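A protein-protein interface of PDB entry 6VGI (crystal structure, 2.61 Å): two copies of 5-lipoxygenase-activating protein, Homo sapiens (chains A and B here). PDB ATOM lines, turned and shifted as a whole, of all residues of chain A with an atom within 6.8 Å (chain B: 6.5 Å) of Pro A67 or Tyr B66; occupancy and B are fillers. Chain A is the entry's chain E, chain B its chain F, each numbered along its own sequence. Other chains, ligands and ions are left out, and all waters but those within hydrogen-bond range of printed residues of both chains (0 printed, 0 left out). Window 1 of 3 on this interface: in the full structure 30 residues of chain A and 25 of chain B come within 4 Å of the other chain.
OD1 of Asp A64 touches CG1 of Val B63, 3.6 Å away. Tyr B66 touches Pro A67. CG of Pro A67 touches CG of Pro B67, 3.999 Å away. Val B22 touches Thr A68 (CG1 to CG2, 3.9 Å). Val A72 touches Val B22.
The backbone carbonyl oxygen of Ser B21 sits close to the side-chain amide oxygen of Asn B25. The side-chain hydroxyl (OG) of Ser B21 is in hydrogen-bond range of the side-chain hydroxyl (OH) of Tyr B66, at 2.6 Å. NH2 of Arg B96 is in hydrogen-bond range of OD1 of Asn B25, at 2.7 Å.
The side-chain amide nitrogen of Asn B25 is in hydrogen-bond range of the side-chain hydroxyl of Thr A68, 2.8 Å away.
Of the 11 printed residues of chain A, 4 touch a printed residue of chain B. Printed residues of chain A that touch a printed residue of chain B: Asp A64, Pro A67, Thr A68 and Val A72. Hydrophobic or aromatic side chains of chain A that line the printed part of chain B: Pro A67 and Val A72. Of the 20 printed residues of chain B, 5 touch a printed residue of chain A. Printed residues of chain B that touch a printed residue of chain A: Val B22, Asn B25, Val B63, Tyr B66 and Pro B67. Hydrophobic or aromatic side chains of chain B within 4 Å of the printed part of chain A: Val B22, Val B63, Tyr B66 and Pro B67. Among the printed residues, 6 pairs touch across the chains. Among the printed residues, no Asp or Glu carboxylate lies within 4 Å of a Lys or Arg side-chain nitrogen of the other chain.
Printed residues of chain B within 4 Å of Asp A64: Val B63 (3.6 Å). Of the printed residues of chain B, Pro A67 touches Tyr B66 (3.95 Å) and Pro B67 (3.999 Å). Of the printed residues of chain B, Thr A68 touches Val B22 and Asn B25. Of the printed residues of chain A, Asn B25 touches Thr A68 (2.8 Å). Tyr B66 touches one residue of chain A. Printed residues of chain A within 4 Å of Pro B67: Pro A67 (3.999 Å). The nearest printed residue of chain A that does not touch Pro B67 is Val A63 (7.0 Å).
Asp A64 touches Val B63, but with the chains exchanged Val A63 does not touch Asp B64 (6.9 Å). Pro A67 touches Tyr B66, but with the chains exchanged Tyr A66 does not touch Pro B67 (7.5 Å). Pro A67 touches its own counterpart, Pro B67. Positions printed for both chains: 62, 63, 64, 65, 66, 67, 68, 69, 70 and 71.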
ATOM      1  N   CYS A  62       4.892   5.134 -24.253  1.00  0.00           N
ATOM      2  CA  CYS A  62       6.007   5.314 -23.322  1.00  0.00           C
ATOM      3  C   CYS A  62       6.728   3.994 -23.056  1.00  0.00           C
ATOM      4  O   CYS A  62       7.957   3.925 -23.138  1.00  0.00           O
ATOM      5  CB  CYS A  62       5.516   5.921 -22.003  1.00  0.00           C
ATOM      6  SG  CYS A  62       5.085   7.672 -22.087  1.00  0.00           S
ATOM      7  N   VAL A  63       5.948   2.957 -22.741  1.00  0.00           N
ATOM      8  CA  VAL A  63       6.463   1.609 -22.480  1.00  0.00           C
ATOM      9  C   VAL A  63       7.262   1.067 -23.667  1.00  0.00           C
ATOM     10  O   VAL A  63       8.342   0.502 -23.482  1.00  0.00           O
ATOM     11  CB  VAL A  63       5.319   0.621 -22.088  1.00  0.00           C
ATOM     12  CG1 VAL A  63       5.799  -0.823 -22.129  1.00  0.00           C
ATOM     13  CG2 VAL A  63       4.773   0.946 -20.702  1.00  0.00           C
ATOM     14  N   ASP A  64       6.737   1.259 -24.877  1.00  0.00           N
ATOM     15  CA  ASP A  64       7.406   0.817 -26.105  1.00  0.00           C
ATOM     16  C   ASP A  64       8.828   1.355 -26.230  1.00  0.00           C
ATOM     17  O   ASP A  64       9.720   0.656 -26.707  1.00  0.00           O
ATOM     18  CB  ASP A  64       6.599   1.224 -27.344  1.00  0.00           C
ATOM     19  CG  ASP A  64       5.299   0.447 -27.493  1.00  0.00           C
ATOM     20  OD1 ASP A  64       4.991  -0.415 -26.639  1.00  0.00           O
ATOM     21  OD2 ASP A  64       4.572   0.710 -28.475  1.00  0.00           O
ATOM     22  N   ALA A  65       9.030   2.595 -25.795  1.00  0.00           N
ATOM     23  CA  ALA A  65      10.304   3.286 -25.967  1.00  0.00           C
ATOM     24  C   ALA A  65      11.263   3.093 -24.795  1.00  0.00           C
ATOM     25  O   ALA A  65      12.467   3.315 -24.937  1.00  0.00           O
ATOM     26  CB  ALA A  65      10.063   4.769 -26.213  1.00  0.00           C
ATOM     27  N   TYR A  66      10.725   2.672 -23.649  1.00  0.00           N
ATOM     28  CA  TYR A  66      11.477   2.613 -22.390  1.00  0.00           C
ATOM     29  C   TYR A  66      12.761   1.764 -22.403  1.00  0.00           C
ATOM     30  O   TYR A  66      13.795   2.230 -21.919  1.00  0.00           O
ATOM     31  CB  TYR A  66      10.562   2.206 -21.229  1.00  0.00           C
ATOM     32  CG  TYR A  66      11.237   2.197 -19.868  1.00  0.00           C
ATOM     33  CD1 TYR A  66      11.727   3.376 -19.300  1.00  0.00           C
ATOM     34  CD2 TYR A  66      11.367   1.013 -19.141  1.00  0.00           C
ATOM     35  CE1 TYR A  66      12.338   3.373 -18.052  1.00  0.00           C
ATOM     36  CE2 TYR A  66      11.976   1.001 -17.890  1.00  0.00           C
ATOM     37  CZ  TYR A  66      12.459   2.185 -17.353  1.00  0.00           C
ATOM     38  OH  TYR A  66      13.063   2.185 -16.118  1.00  0.00           O
ATOM     39  N   PRO A  67      12.709   0.527 -22.946  1.00  0.00           N
ATOM     40  CA  PRO A  67      13.946  -0.268 -22.955  1.00  0.00           C
ATOM     41  C   PRO A  67      15.033   0.295 -23.876  1.00  0.00           C
ATOM     42  O   PRO A  67      16.222   0.124 -23.591  1.00  0.00           O
ATOM     43  CB  PRO A  67      13.481  -1.647 -23.440  1.00  0.00           C
ATOM     44  CG  PRO A  67      12.015  -1.672 -23.173  1.00  0.00           C
ATOM     45  CD  PRO A  67      11.558  -0.268 -23.410  1.00  0.00           C
ATOM     46  N   THR A  68      14.629   0.956 -24.960  1.00  0.00           N
ATOM     47  CA  THR A  68      15.570   1.652 -25.843  1.00  0.00           C
ATOM     48  C   THR A  68      16.257   2.801 -25.095  1.00  0.00           C
ATOM     49  O   THR A  68      17.470   2.986 -25.214  1.00  0.00           O
ATOM     50  CB  THR A  68      14.877   2.180 -27.124  1.00  0.00           C
ATOM     51  OG1 THR A  68      14.248   1.090 -27.813  1.00  0.00           O
ATOM     52  CG2 THR A  68      15.884   2.844 -28.059  1.00  0.00           C
ATOM     53  N   PHE A  69      15.478   3.553 -24.318  1.00  0.00           N
ATOM     54  CA  PHE A  69      16.013   4.623 -23.478  1.00  0.00           C
ATOM     55  C   PHE A  69      16.999   4.080 -22.449  1.00  0.00           C
ATOM     56  O   PHE A  69      18.099   4.614 -22.285  1.00  0.00           O
ATOM     57  CB  PHE A  69      14.883   5.379 -22.768  1.00  0.00           C
ATOM     58  CG  PHE A  69      15.340   6.182 -21.575  1.00  0.00           C
ATOM     59  CD1 PHE A  69      16.172   7.291 -21.736  1.00  0.00           C
ATOM     60  CD2 PHE A  69      14.940   5.827 -20.289  1.00  0.00           C
ATOM     61  CE1 PHE A  69      16.599   8.031 -20.633  1.00  0.00           C
ATOM     62  CE2 PHE A  69      15.360   6.560 -19.178  1.00  0.00           C
ATOM     63  CZ  PHE A  69      16.189   7.666 -19.350  1.00  0.00           C
ATOM     64  N   LEU A  70      16.589   3.017 -21.761  1.00  0.00           N
ATOM     65  CA  LEU A  70      17.381   2.423 -20.695  1.00  0.00           C
ATOM     66  C   LEU A  70      18.688   1.864 -21.251  1.00  0.00           C
ATOM     67  O   LEU A  70      19.727   1.929 -20.596  1.00  0.00           O
ATOM     68  CB  LEU A  70      16.568   1.337 -19.983  1.00  0.00           C
ATOM     69  CG  LEU A  70      16.527   1.317 -18.449  1.00  0.00           C
ATOM     70  CD1 LEU A  70      16.059   2.651 -17.861  1.00  0.00           C
ATOM     71  CD2 LEU A  70      15.633   0.186 -17.959  1.00  0.00           C
ATOM     72  N   ALA A  71      18.633   1.342 -22.474  1.00  0.00           N
ATOM     73  CA  ALA A  71      19.819   0.821 -23.150  1.00  0.00           C
ATOM     74  C   ALA A  71      20.849   1.912 -23.440  1.00  0.00           C
ATOM     75  O   ALA A  71      22.025   1.743 -23.124  1.00  0.00           O
ATOM     76  CB  ALA A  71      19.434   0.088 -24.426  1.00  0.00           C
ATOM     77  N   VAL A  72      20.412   3.027 -24.032  1.00  0.00           N
ATOM     78  CA  VAL A  72      21.337   4.122 -24.369  1.00  0.00           C
ATOM     79  C   VAL A  72      21.787   4.936 -23.161  1.00  0.00           C
ATOM     80  O   VAL A  72      22.906   5.450 -23.146  1.00  0.00           O
ATOM     81  CB  VAL A  72      20.811   5.074 -25.488  1.00  0.00           C
ATOM     82  CG1 VAL A  72      20.768   4.358 -26.823  1.00  0.00           C
ATOM     83  CG2 VAL A  72      19.451   5.679 -25.135  1.00  0.00           C
ATOM     84  N   VAL B  17      26.335  -4.026 -31.078  1.00  0.00           N
ATOM     85  CA  VAL B  17      25.109  -4.678 -31.551  1.00  0.00           C
ATOM     86  C   VAL B  17      23.862  -4.112 -30.851  1.00  0.00           C
ATOM     87  O   VAL B  17      22.798  -4.008 -31.460  1.00  0.00           O
ATOM     88  CB  VAL B  17      25.199  -6.251 -31.511  1.00  0.00           C
ATOM     89  CG1 VAL B  17      25.236  -6.788 -30.092  1.00  0.00           C
ATOM     90  CG2 VAL B  17      24.053  -6.887 -32.286  1.00  0.00           C
ATOM     91  N   THR B  18      24.012  -3.720 -29.587  1.00  0.00           N
ATOM     92  CA  THR B  18      22.940  -3.046 -28.851  1.00  0.00           C
ATOM     93  C   THR B  18      22.629  -1.691 -29.488  1.00  0.00           C
ATOM     94  O   THR B  18      21.461  -1.330 -29.662  1.00  0.00           O
ATOM     95  CB  THR B  18      23.302  -2.863 -27.361  1.00  0.00           C
ATOM     96  OG1 THR B  18      23.572  -4.143 -26.778  1.00  0.00           O
ATOM     97  CG2 THR B  18      22.164  -2.200 -26.594  1.00  0.00           C
ATOM     98  N   LEU B  19      23.678  -0.958 -29.852  1.00  0.00           N
ATOM     99  CA  LEU B  19      23.515   0.343 -30.493  1.00  0.00           C
ATOM    100  C   LEU B  19      22.884   0.241 -31.880  1.00  0.00           C
ATOM    101  O   LEU B  19      22.118   1.121 -32.277  1.00  0.00           O
ATOM    102  CB  LEU B  19      24.841   1.104 -30.548  1.00  0.00           C
ATOM    103  CG  LEU B  19      25.385   1.674 -29.232  1.00  0.00           C
ATOM    104  CD1 LEU B  19      26.732   2.321 -29.484  1.00  0.00           C
ATOM    105  CD2 LEU B  19      24.424   2.671 -28.596  1.00  0.00           C
ATOM    106  N   SER B  21      20.716  -2.168 -32.699  1.00  0.00           N
ATOM    107  CA  SER B  21      19.315  -2.475 -32.395  1.00  0.00           C
ATOM    108  C   SER B  21      18.520  -1.219 -32.026  1.00  0.00           C
ATOM    109  O   SER B  21      17.325  -1.131 -32.316  1.00  0.00           O
ATOM    110  CB  SER B  21      19.205  -3.529 -31.288  1.00  0.00           C
ATOM    111  OG  SER B  21      19.512  -2.989 -30.015  1.00  0.00           O
ATOM    112  N   VAL B  22      19.197  -0.259 -31.392  1.00  0.00           N
ATOM    113  CA  VAL B  22      18.609   1.041 -31.049  1.00  0.00           C
ATOM    114  C   VAL B  22      18.272   1.846 -32.308  1.00  0.00           C
ATOM    115  O   VAL B  22      17.188   2.424 -32.406  1.00  0.00           O
ATOM    116  CB  VAL B  22      19.530   1.854 -30.095  1.00  0.00           C
ATOM    117  CG1 VAL B  22      19.167   3.339 -30.095  1.00  0.00           C
ATOM    118  CG2 VAL B  22      19.460   1.291 -28.679  1.00  0.00           C
ATOM    119  N   ASN B  25      15.274   0.088 -33.752  1.00  0.00           N
ATOM    120  CA  ASN B  25      14.074   0.455 -32.994  1.00  0.00           C
ATOM    121  C   ASN B  25      13.523   1.816 -33.408  1.00  0.00           C
ATOM    122  O   ASN B  25      12.314   1.975 -33.603  1.00  0.00           O
ATOM    123  CB  ASN B  25      14.358   0.452 -31.488  1.00  0.00           C
ATOM    124  CG  ASN B  25      14.491  -0.948 -30.914  1.00  0.00           C
ATOM    125  OD1 ASN B  25      14.390  -1.946 -31.630  1.00  0.00           O
ATOM    126  ND2 ASN B  25      14.722  -1.027 -29.609  1.00  0.00           N
ATOM    127  N   ASN B  61       4.972  -6.190 -31.911  1.00  0.00           N
ATOM    128  CA  ASN B  61       5.607  -7.501 -31.780  1.00  0.00           C
ATOM    129  C   ASN B  61       7.120  -7.404 -31.550  1.00  0.00           C
ATOM    130  O   ASN B  61       7.657  -8.076 -30.667  1.00  0.00           O
ATOM    131  CB  ASN B  61       5.311  -8.366 -33.012  1.00  0.00           C
ATOM    132  CG  ASN B  61       3.817  -8.564 -33.254  1.00  0.00           C
ATOM    133  OD1 ASN B  61       2.997  -8.440 -32.342  1.00  0.00           O
ATOM    134  ND2 ASN B  61       3.461  -8.873 -34.495  1.00  0.00           N
ATOM    135  N   CYS B  62       7.787  -6.565 -32.348  1.00  0.00           N
ATOM    136  CA  CYS B  62       9.226  -6.302 -32.218  1.00  0.00           C
ATOM    137  C   CYS B  62       9.594  -5.705 -30.858  1.00  0.00           C
ATOM    138  O   CYS B  62      10.642  -6.022 -30.293  1.00  0.00           O
ATOM    139  CB  CYS B  62       9.699  -5.358 -33.327  1.00  0.00           C
ATOM    140  SG  CYS B  62       9.761  -6.080 -34.977  1.00  0.00           S
ATOM    141  N   VAL B  63       8.726  -4.831 -30.355  1.00  0.00           N
ATOM    142  CA  VAL B  63       8.905  -4.184 -29.062  1.00  0.00           C
ATOM    143  C   VAL B  63       8.675  -5.175 -27.921  1.00  0.00           C
ATOM    144  O   VAL B  63       9.433  -5.194 -26.949  1.00  0.00           O
ATOM    145  CB  VAL B  63       7.984  -2.935 -28.939  1.00  0.00           C
ATOM    146  CG1 VAL B  63       7.671  -2.591 -27.484  1.00  0.00           C
ATOM    147  CG2 VAL B  63       8.612  -1.746 -29.659  1.00  0.00           C
ATOM    148  N   ASP B  64       7.643  -6.007 -28.059  1.00  0.00           N
ATOM    149  CA  ASP B  64       7.305  -7.021 -27.056  1.00  0.00           C
ATOM    150  C   ASP B  64       8.422  -8.041 -26.826  1.00  0.00           C
ATOM    151  O   ASP B  64       8.514  -8.632 -25.749  1.00  0.00           O
ATOM    152  CB  ASP B  64       6.014  -7.752 -27.441  1.00  0.00           C
ATOM    153  CG  ASP B  64       4.769  -6.895 -27.261  1.00  0.00           C
ATOM    154  OD1 ASP B  64       4.892  -5.704 -26.896  1.00  0.00           O
ATOM    155  OD2 ASP B  64       3.659  -7.418 -27.493  1.00  0.00           O
ATOM    156  N   ALA B  65       9.263  -8.239 -27.837  1.00  0.00           N
ATOM    157  CA  ALA B  65      10.342  -9.220 -27.759  1.00  0.00           C
ATOM    158  C   ALA B  65      11.720  -8.606 -27.494  1.00  0.00           C
ATOM    159  O   ALA B  65      12.703  -9.336 -27.342  1.00  0.00           O
ATOM    160  CB  ALA B  65      10.373 -10.071 -29.020  1.00  0.00           C
ATOM    161  N   TYR B  66      11.791  -7.278 -27.428  1.00  0.00           N
ATOM    162  CA  TYR B  66      13.074  -6.586 -27.287  1.00  0.00           C
ATOM    163  C   TYR B  66      13.785  -6.790 -25.939  1.00  0.00           C
ATOM    164  O   TYR B  66      14.977  -7.105 -25.930  1.00  0.00           O
ATOM    165  CB  TYR B  66      12.952  -5.096 -27.628  1.00  0.00           C
ATOM    166  CG  TYR B  66      14.286  -4.373 -27.715  1.00  0.00           C
ATOM    167  CD1 TYR B  66      15.223  -4.714 -28.693  1.00  0.00           C
ATOM    168  CD2 TYR B  66      14.602  -3.342 -26.832  1.00  0.00           C
ATOM    169  CE1 TYR B  66      16.447  -4.055 -28.782  1.00  0.00           C
ATOM    170  CE2 TYR B  66      15.825  -2.672 -26.916  1.00  0.00           C
ATOM    171  CZ  TYR B  66      16.741  -3.034 -27.893  1.00  0.00           C
ATOM    172  OH  TYR B  66      17.952  -2.381 -27.984  1.00  0.00           O
ATOM    173  N   PRO B  67      13.073  -6.608 -24.803  1.00  0.00           N
ATOM    174  CA  PRO B  67      13.743  -6.815 -23.512  1.00  0.00           C
ATOM    175  C   PRO B  67      14.294  -8.236 -23.349  1.00  0.00           C
ATOM    176  O   PRO B  67      15.420  -8.408 -22.872  1.00  0.00           O
ATOM    177  CB  PRO B  67      12.632  -6.544 -22.491  1.00  0.00           C
ATOM    178  CG  PRO B  67      11.676  -5.657 -23.202  1.00  0.00           C
ATOM    179  CD  PRO B  67      11.685  -6.140 -24.618  1.00  0.00           C
ATOM    180  N   THR B  68      13.507  -9.231 -23.757  1.00  0.00           N
ATOM    181  CA  THR B  68      13.922 -10.634 -23.724  1.00  0.00           C
ATOM    182  C   THR B  68      15.199 -10.855 -24.538  1.00  0.00           C
ATOM    183  O   THR B  68      16.156 -11.451 -24.039  1.00  0.00           O
ATOM    184  CB  THR B  68      12.783 -11.571 -24.203  1.00  0.00           C
ATOM    185  OG1 THR B  68      11.710 -11.536 -23.254  1.00  0.00           O
ATOM    186  CG2 THR B  68      13.268 -13.010 -24.345  1.00  0.00           C
ATOM    187  N   PHE B  69      15.218 -10.359 -25.777  1.00  0.00           N
ATOM    188  CA  PHE B  69      16.410 -10.435 -26.622  1.00  0.00           C
ATOM    189  C   PHE B  69      17.607  -9.755 -25.960  1.00  0.00           C
ATOM    190  O   PHE B  69      18.716 -10.298 -25.962  1.00  0.00           O
ATOM    191  CB  PHE B  69      16.154  -9.830 -28.008  1.00  0.00           C
ATOM    192  CG  PHE B  69      17.415  -9.461 -28.759  1.00  0.00           C
ATOM    193  CD1 PHE B  69      18.305 -10.444 -29.190  1.00  0.00           C
ATOM    194  CD2 PHE B  69      17.706  -8.130 -29.038  1.00  0.00           C
ATOM    195  CE1 PHE B  69      19.468 -10.104 -29.881  1.00  0.00           C
ATOM    196  CE2 PHE B  69      18.869  -7.778 -29.733  1.00  0.00           C
ATOM    197  CZ  PHE B  69      19.750  -8.765 -30.152  1.00  0.00           C
ATOM    198  N   LEU B  70      17.373  -8.571 -25.397  1.00  0.00           N
ATOM    199  CA  LEU B  70      18.425  -7.810 -24.738  1.00  0.00           C
ATOM    200  C   LEU B  70      18.970  -8.582 -23.538  1.00  0.00           C
ATOM    201  O   LEU B  70      20.183  -8.613 -23.315  1.00  0.00           O
ATOM    202  CB  LEU B  70      17.908  -6.427 -24.327  1.00  0.00           C
ATOM    203  CG  LEU B  70      18.835  -5.230 -24.568  1.00  0.00           C
ATOM    204  CD1 LEU B  70      19.265  -5.132 -26.031  1.00  0.00           C
ATOM    205  CD2 LEU B  70      18.165  -3.937 -24.132  1.00  0.00           C
ATOM    206  N   ALA B  71      18.068  -9.225 -22.796  1.00  0.00           N
ATOM    207  CA  ALA B  71      18.434 -10.044 -21.641  1.00  0.00           C
ATOM    208  C   ALA B  71      19.329 -11.224 -22.021  1.00  0.00           C
ATOM    209  O   ALA B  71      20.402 -11.393 -21.442  1.00  0.00           O
ATOM    210  CB  ALA B  71      17.184 -10.529 -20.899  1.00  0.00           C
ATOM    211  N   TYR B  92      19.819 -11.906 -35.198  1.00  0.00           N
ATOM    212  CA  TYR B  92      18.490 -11.539 -34.701  1.00  0.00           C
ATOM    213  C   TYR B  92      18.011 -10.218 -35.302  1.00  0.00           C
ATOM    214  O   TYR B  92      16.834 -10.071 -35.632  1.00  0.00           O
ATOM    215  CB  TYR B  92      18.487 -11.458 -33.169  1.00  0.00           C
ATOM    216  CG  TYR B  92      17.130 -11.165 -32.554  1.00  0.00           C
ATOM    217  CD1 TYR B  92      16.229 -12.195 -32.285  1.00  0.00           C
ATOM    218  CD2 TYR B  92      16.750  -9.858 -32.235  1.00  0.00           C
ATOM    219  CE1 TYR B  92      14.981 -11.931 -31.718  1.00  0.00           C
ATOM    220  CE2 TYR B  92      15.504  -9.586 -31.667  1.00  0.00           C
ATOM    221  CZ  TYR B  92      14.628 -10.626 -31.412  1.00  0.00           C
ATOM    222  OH  TYR B  92      13.399 -10.367 -30.852  1.00  0.00           O
ATOM    223  N   LEU B  93      18.934  -9.267 -35.438  1.00  0.00           N
ATOM    224  CA  LEU B  93      18.634  -7.961 -36.025  1.00  0.00           C
ATOM    225  C   LEU B  93      18.254  -8.068 -37.498  1.00  0.00           C
ATOM    226  O   LEU B  93      17.334  -7.385 -37.954  1.00  0.00           O
ATOM    227  CB  LEU B  93      19.813  -6.999 -35.837  1.00  0.00           C
ATOM    228  CG  LEU B  93      19.868  -6.098 -34.595  1.00  0.00           C
ATOM    229  CD1 LEU B  93      19.461  -6.794 -33.298  1.00  0.00           C
ATOM    230  CD2 LEU B  93      21.256  -5.514 -34.450  1.00  0.00           C
ATOM    231  N   ARG B  96      14.760  -9.578 -37.618  1.00  0.00           N
ATOM    232  CA  ARG B  96      13.804  -8.510 -37.291  1.00  0.00           C
ATOM    233  C   ARG B  96      13.514  -7.624 -38.494  1.00  0.00           C
ATOM    234  O   ARG B  96      12.360  -7.290 -38.763  1.00  0.00           O
ATOM    235  CB  ARG B  96      14.322  -7.620 -36.161  1.00  0.00           C
ATOM    236  CG  ARG B  96      14.121  -8.165 -34.767  1.00  0.00           C
ATOM    237  CD  ARG B  96      13.752  -7.064 -33.777  1.00  0.00           C
ATOM    238  NE  ARG B  96      14.649  -5.914 -33.857  1.00  0.00           N
ATOM    239  CZ  ARG B  96      14.653  -4.896 -33.002  1.00  0.00           C
ATOM    240  NH1 ARG B  96      13.810  -4.873 -31.976  1.00  0.00           N
ATOM    241  NH2 ARG B  96      15.511  -3.899 -33.173  1.00  0.00           N
